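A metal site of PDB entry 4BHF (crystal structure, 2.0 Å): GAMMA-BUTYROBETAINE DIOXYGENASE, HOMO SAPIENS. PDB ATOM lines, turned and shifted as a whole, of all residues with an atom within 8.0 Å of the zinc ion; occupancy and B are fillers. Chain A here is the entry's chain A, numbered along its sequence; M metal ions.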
ATOM      1  N   LEU A  34      15.612  29.255 -20.109  1.00  0.00           N
ATOM      2  CA  LEU A  34      16.162  28.164 -20.907  1.00  0.00           C
ATOM      3  C   LEU A  34      15.486  26.856 -20.592  1.00  0.00           C
ATOM      4  O   LEU A  34      15.081  26.146 -21.516  1.00  0.00           O
ATOM      5  CB  LEU A  34      17.656  28.008 -20.659  1.00  0.00           C
ATOM      6  CG  LEU A  34      18.532  29.135 -21.229  1.00  0.00           C
ATOM      7  CD1 LEU A  34      19.915  29.043 -20.569  1.00  0.00           C
ATOM      8  CD2 LEU A  34      18.618  29.035 -22.756  1.00  0.00           C
ATOM      9  N   ARG A  35      15.386  26.511 -19.312  1.00  0.00           N
ATOM     10  CA  ARG A  35      14.719  25.239 -18.925  1.00  0.00           C
ATOM     11  C   ARG A  35      13.252  25.211 -19.387  1.00  0.00           C
ATOM     12  O   ARG A  35      12.743  24.192 -19.906  1.00  0.00           O
ATOM     13  CB  ARG A  35      14.764  25.008 -17.414  1.00  0.00           C
ATOM     14  CG  ARG A  35      14.053  23.720 -16.925  1.00  0.00           C
ATOM     15  CD  ARG A  35      14.764  22.458 -17.461  1.00  0.00           C
ATOM     16  NE  ARG A  35      14.076  21.181 -17.247  1.00  0.00           N
ATOM     17  CZ  ARG A  35      13.153  20.665 -18.055  1.00  0.00           C
ATOM     18  NH1 ARG A  35      12.784  21.312 -19.155  1.00  0.00           N
ATOM     19  NH2 ARG A  35      12.625  19.470 -17.790  1.00  0.00           N
ATOM     20  N   ASP A  36      12.574  26.351 -19.186  1.00  0.00           N
ATOM     21  CA  ASP A  36      11.160  26.527 -19.653  1.00  0.00           C
ATOM     22  C   ASP A  36      11.007  26.266 -21.128  1.00  0.00           C
ATOM     23  O   ASP A  36       9.978  25.802 -21.587  1.00  0.00           O
ATOM     24  CB  ASP A  36      10.675  27.952 -19.334  1.00  0.00           C
ATOM     25  CG  ASP A  36       9.230  28.182 -19.753  1.00  0.00           C
ATOM     26  OD1 ASP A  36       8.381  27.359 -19.389  1.00  0.00           O
ATOM     27  OD2 ASP A  36       8.974  29.183 -20.477  1.00  0.00           O
ATOM     28  N   ASN A  37      12.060  26.553 -21.883  1.00  0.00           N
ATOM     29  CA  ASN A  37      11.981  26.477 -23.327  1.00  0.00           C
ATOM     30  C   ASN A  37      12.857  25.424 -23.970  1.00  0.00           C
ATOM     31  O   ASN A  37      13.167  25.504 -25.150  1.00  0.00           O
ATOM     32  CB  ASN A  37      12.266  27.857 -23.880  1.00  0.00           C
ATOM     33  CG  ASN A  37      11.145  28.799 -23.580  1.00  0.00           C
ATOM     34  OD1 ASN A  37      10.023  28.547 -24.020  1.00  0.00           O
ATOM     35  ND2 ASN A  37      11.396  29.851 -22.789  1.00  0.00           N
ATOM     36  N   CYS A  38      13.172  24.389 -23.199  1.00  0.00           N
ATOM     37  CA  CYS A  38      13.859  23.215 -23.719  1.00  0.00           C
ATOM     38  C   CYS A  38      13.085  22.656 -24.927  1.00  0.00           C
ATOM     39  O   CYS A  38      11.867  22.440 -24.831  1.00  0.00           O
ATOM     40  CB  CYS A  38      13.986  22.149 -22.623  1.00  0.00           C
ATOM     41  SG  CYS A  38      14.719  20.579 -23.228  1.00  0.00           S
ATOM     42  N   PRO A  39      13.747  22.496 -26.074  1.00  0.00           N
ATOM     43  CA  PRO A  39      13.065  21.986 -27.260  1.00  0.00           C
ATOM     44  C   PRO A  39      12.967  20.479 -27.406  1.00  0.00           C
ATOM     45  O   PRO A  39      12.554  20.018 -28.445  1.00  0.00           O
ATOM     46  CB  PRO A  39      13.903  22.557 -28.420  1.00  0.00           C
ATOM     47  CG  PRO A  39      15.256  22.764 -27.860  1.00  0.00           C
ATOM     48  CD  PRO A  39      15.073  23.082 -26.400  1.00  0.00           C
ATOM     49  N   CYS A  40      13.354  19.690 -26.406  1.00  0.00           N
ATOM     50  CA  CYS A  40      13.330  18.254 -26.544  1.00  0.00           C
ATOM     51  C   CYS A  40      11.867  17.761 -26.619  1.00  0.00           C
ATOM     52  O   CYS A  40      10.934  18.472 -26.229  1.00  0.00           O
ATOM     53  CB  CYS A  40      14.076  17.575 -25.371  1.00  0.00           C
ATOM     54  SG  CYS A  40      13.088  17.267 -23.875  1.00  0.00           S
ATOM     55  N   SER A  41      11.673  16.535 -27.069  1.00  0.00           N
ATOM     56  CA  SER A  41      10.333  15.991 -27.283  1.00  0.00           C
ATOM     57  C   SER A  41       9.547  15.761 -25.988  1.00  0.00           C
ATOM     58  O   SER A  41       8.313  15.675 -26.030  1.00  0.00           O
ATOM     59  CB  SER A  41      10.395  14.720 -28.125  1.00  0.00           C
ATOM     60  OG  SER A  41      10.858  13.603 -27.379  1.00  0.00           O
ATOM     61  N   ASP A  42      10.238  15.702 -24.843  1.00  0.00           N
ATOM     62  CA  ASP A  42       9.540  15.663 -23.554  1.00  0.00           C
ATOM     63  C   ASP A  42       8.836  16.999 -23.262  1.00  0.00           C
ATOM     64  O   ASP A  42       7.694  17.023 -22.769  1.00  0.00           O
ATOM     65  CB  ASP A  42      10.488  15.353 -22.396  1.00  0.00           C
ATOM     66  CG  ASP A  42      11.001  13.911 -22.400  1.00  0.00           C
ATOM     67  OD1 ASP A  42      10.542  13.086 -23.197  1.00  0.00           O
ATOM     68  OD2 ASP A  42      11.856  13.596 -21.548  1.00  0.00           O
ATOM     69  N   CYS A  43       9.498  18.094 -23.612  1.00  0.00           N
ATOM     70  CA  CYS A  43       9.119  19.423 -23.195  1.00  0.00           C
ATOM     71  C   CYS A  43       8.380  20.169 -24.243  1.00  0.00           C
ATOM     72  O   CYS A  43       7.815  21.214 -23.967  1.00  0.00           O
ATOM     73  CB  CYS A  43      10.402  20.202 -22.868  1.00  0.00           C
ATOM     74  SG  CYS A  43      11.250  19.539 -21.455  1.00  0.00           S
ATOM     75  N   TYR A  44       8.390  19.658 -25.466  1.00  0.00           N
ATOM     76  CA  TYR A  44       7.988  20.461 -26.615  1.00  0.00           C
ATOM     77  C   TYR A  44       7.441  19.581 -27.723  1.00  0.00           C
ATOM     78  O   TYR A  44       8.127  18.651 -28.169  1.00  0.00           O
ATOM     79  CB  TYR A  44       9.214  21.228 -27.126  1.00  0.00           C
ATOM     80  CG  TYR A  44       8.846  22.366 -28.055  1.00  0.00           C
ATOM     81  CD1 TYR A  44       8.433  23.597 -27.557  1.00  0.00           C
ATOM     82  CD2 TYR A  44       8.842  22.173 -29.436  1.00  0.00           C
ATOM     83  CE1 TYR A  44       8.068  24.625 -28.407  1.00  0.00           C
ATOM     84  CE2 TYR A  44       8.486  23.204 -30.288  1.00  0.00           C
ATOM     85  CZ  TYR A  44       8.083  24.411 -29.774  1.00  0.00           C
ATOM     86  OH  TYR A  44       7.706  25.401 -30.638  1.00  0.00           O
ATOM     87  N   LEU A  53       5.869  21.103 -21.478  1.00  0.00           N
ATOM     88  CA  LEU A  53       6.305  21.350 -20.121  1.00  0.00           C
ATOM     89  C   LEU A  53       5.269  22.145 -19.295  1.00  0.00           C
ATOM     90  O   LEU A  53       4.818  23.200 -19.709  1.00  0.00           O
ATOM     91  CB  LEU A  53       7.610  22.122 -20.116  1.00  0.00           C
ATOM     92  CG  LEU A  53       8.339  22.224 -18.797  1.00  0.00           C
ATOM     93  CD1 LEU A  53       8.924  20.889 -18.417  1.00  0.00           C
ATOM     94  CD2 LEU A  53       9.470  23.228 -18.930  1.00  0.00           C
ATOM     95  N   TRP A  78      20.990  19.799 -16.477  1.00  0.00           N
ATOM     96  CA  TRP A  78      20.264  20.419 -15.389  1.00  0.00           C
ATOM     97  C   TRP A  78      20.444  19.625 -14.069  1.00  0.00           C
ATOM     98  O   TRP A  78      20.720  18.438 -14.074  1.00  0.00           O
ATOM     99  CB  TRP A  78      18.796  20.488 -15.794  1.00  0.00           C
ATOM    100  CG  TRP A  78      18.529  21.436 -16.954  1.00  0.00           C
ATOM    101  CD1 TRP A  78      18.113  21.098 -18.209  1.00  0.00           C
ATOM    102  CD2 TRP A  78      18.653  22.861 -16.957  1.00  0.00           C
ATOM    103  NE1 TRP A  78      17.987  22.202 -18.988  1.00  0.00           N
ATOM    104  CE2 TRP A  78      18.290  23.303 -18.248  1.00  0.00           C
ATOM    105  CE3 TRP A  78      19.025  23.801 -15.999  1.00  0.00           C
ATOM    106  CZ2 TRP A  78      18.324  24.656 -18.609  1.00  0.00           C
ATOM    107  CZ3 TRP A  78      19.024  25.172 -16.349  1.00  0.00           C
ATOM    108  CH2 TRP A  78      18.683  25.564 -17.656  1.00  0.00           C
ATOM    109  N   HIS A  82      17.899  16.316 -16.388  1.00  0.00           N
ATOM    110  CA  HIS A  82      17.369  16.678 -17.686  1.00  0.00           C
ATOM    111  C   HIS A  82      18.478  17.284 -18.561  1.00  0.00           C
ATOM    112  O   HIS A  82      19.448  17.919 -18.068  1.00  0.00           O
ATOM    113  CB  HIS A  82      16.184  17.654 -17.550  1.00  0.00           C
ATOM    114  CG  HIS A  82      15.335  17.709 -18.782  1.00  0.00           C
ATOM    115  ND1 HIS A  82      14.409  16.734 -19.090  1.00  0.00           N
ATOM    116  CD2 HIS A  82      15.270  18.620 -19.769  1.00  0.00           C
ATOM    117  CE1 HIS A  82      13.824  17.038 -20.226  1.00  0.00           C
ATOM    118  NE2 HIS A  82      14.324  18.179 -20.659  1.00  0.00           N
ATOM    119  N   TYR A  83      18.332  17.108 -19.865  1.00  0.00           N
ATOM    120  CA  TYR A  83      19.352  17.526 -20.807  1.00  0.00           C
ATOM    121  C   TYR A  83      18.729  18.390 -21.898  1.00  0.00           C
ATOM    122  O   TYR A  83      17.653  18.091 -22.342  1.00  0.00           O
ATOM    123  CB  TYR A  83      20.021  16.281 -21.390  1.00  0.00           C
ATOM    124  CG  TYR A  83      20.932  16.591 -22.516  1.00  0.00           C
ATOM    125  CD1 TYR A  83      22.094  17.332 -22.313  1.00  0.00           C
ATOM    126  CD2 TYR A  83      20.639  16.171 -23.821  1.00  0.00           C
ATOM    127  CE1 TYR A  83      22.933  17.639 -23.359  1.00  0.00           C
ATOM    128  CE2 TYR A  83      21.479  16.473 -24.876  1.00  0.00           C
ATOM    129  CZ  TYR A  83      22.627  17.203 -24.643  1.00  0.00           C
ATOM    130  OH  TYR A  83      23.476  17.508 -25.699  1.00  0.00           O
ATOM    131  N   SER A  84      19.396  19.489 -22.285  1.00  0.00           N
ATOM    132  CA  SER A  84      18.840  20.401 -23.321  1.00  0.00           C
ATOM    133  C   SER A  84      19.881  20.875 -24.365  1.00  0.00           C
ATOM    134  O   SER A  84      21.038  21.145 -24.017  1.00  0.00           O
ATOM    135  CB  SER A  84      18.188  21.656 -22.673  1.00  0.00           C
ATOM    136  OG  SER A  84      17.278  21.380 -21.613  1.00  0.00           O
ATOM    137  N   GLU A  85      19.472  20.995 -25.628  1.00  0.00           N
ATOM    138  CA  GLU A  85      20.300  21.570 -26.696  1.00  0.00           C
ATOM    139  C   GLU A  85      19.597  22.799 -27.252  1.00  0.00           C
ATOM    140  O   GLU A  85      18.383  22.756 -27.518  1.00  0.00           O
ATOM    141  CB  GLU A  85      20.532  20.548 -27.821  1.00  0.00           C
ATOM    142  CG  GLU A  85      21.171  19.268 -27.308  1.00  0.00           C
ATOM    143  CD  GLU A  85      21.590  18.297 -28.409  1.00  0.00           C
ATOM    144  OE1 GLU A  85      21.293  18.538 -29.587  1.00  0.00           O
ATOM    145  OE2 GLU A  85      22.214  17.279 -28.043  1.00  0.00           O
ATOM    146  N   PHE A  86      20.338  23.894 -27.412  1.00  0.00           N
ATOM    147  CA  PHE A  86      19.834  25.107 -28.018  1.00  0.00           C
ATOM    148  C   PHE A  86      20.703  25.542 -29.176  1.00  0.00           C
ATOM    149  O   PHE A  86      21.940  25.544 -29.071  1.00  0.00           O
ATOM    150  CB  PHE A  86      19.762  26.246 -27.003  1.00  0.00           C
ATOM    151  CG  PHE A  86      18.939  25.934 -25.777  1.00  0.00           C
ATOM    152  CD1 PHE A  86      19.536  25.373 -24.660  1.00  0.00           C
ATOM    153  CD2 PHE A  86      17.578  26.227 -25.750  1.00  0.00           C
ATOM    154  CE1 PHE A  86      18.801  25.072 -23.530  1.00  0.00           C
ATOM    155  CE2 PHE A  86      16.842  25.941 -24.595  1.00  0.00           C
ATOM    156  CZ  PHE A  86      17.444  25.352 -23.507  1.00  0.00           C
HETATM  157 ZN    ZN M   1      13.380  18.933 -22.343  1.00  0.00          ZN
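A ring nitrogen (NE2) of His 82 is bound to the zinc ion. The zinc ion is bound by the side-chain sulfur (SG) of Cys 40, 2.3 Å away. SG of Cys 38 binds the zinc ion (2.3 Å). The side-chain sulfur (SG) of Cys 43 is bound to the zinc ion.
SG of Cys 43 sits close to NH1 of Arg 35 (3.3 Å). OG of Ser 84 lies close to SG of Cys 38 (3.1 Å). The backbone carbonyl oxygen of Cys 43 is in hydrogen-bond range of the backbone NH of Leu 53, 3.2 Å away. The side-chain sulfur (SG) of Cys 40 lies close to the backbone NH (N) of Asp 42, 3.4 Å away.
Four residues have an atom within 4 Å of the zinc ion: Cys 38, Cys 40, Cys 43 and His 82. Along chain A the residues within 4 Å of the zinc ion span positions 38 to 82.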
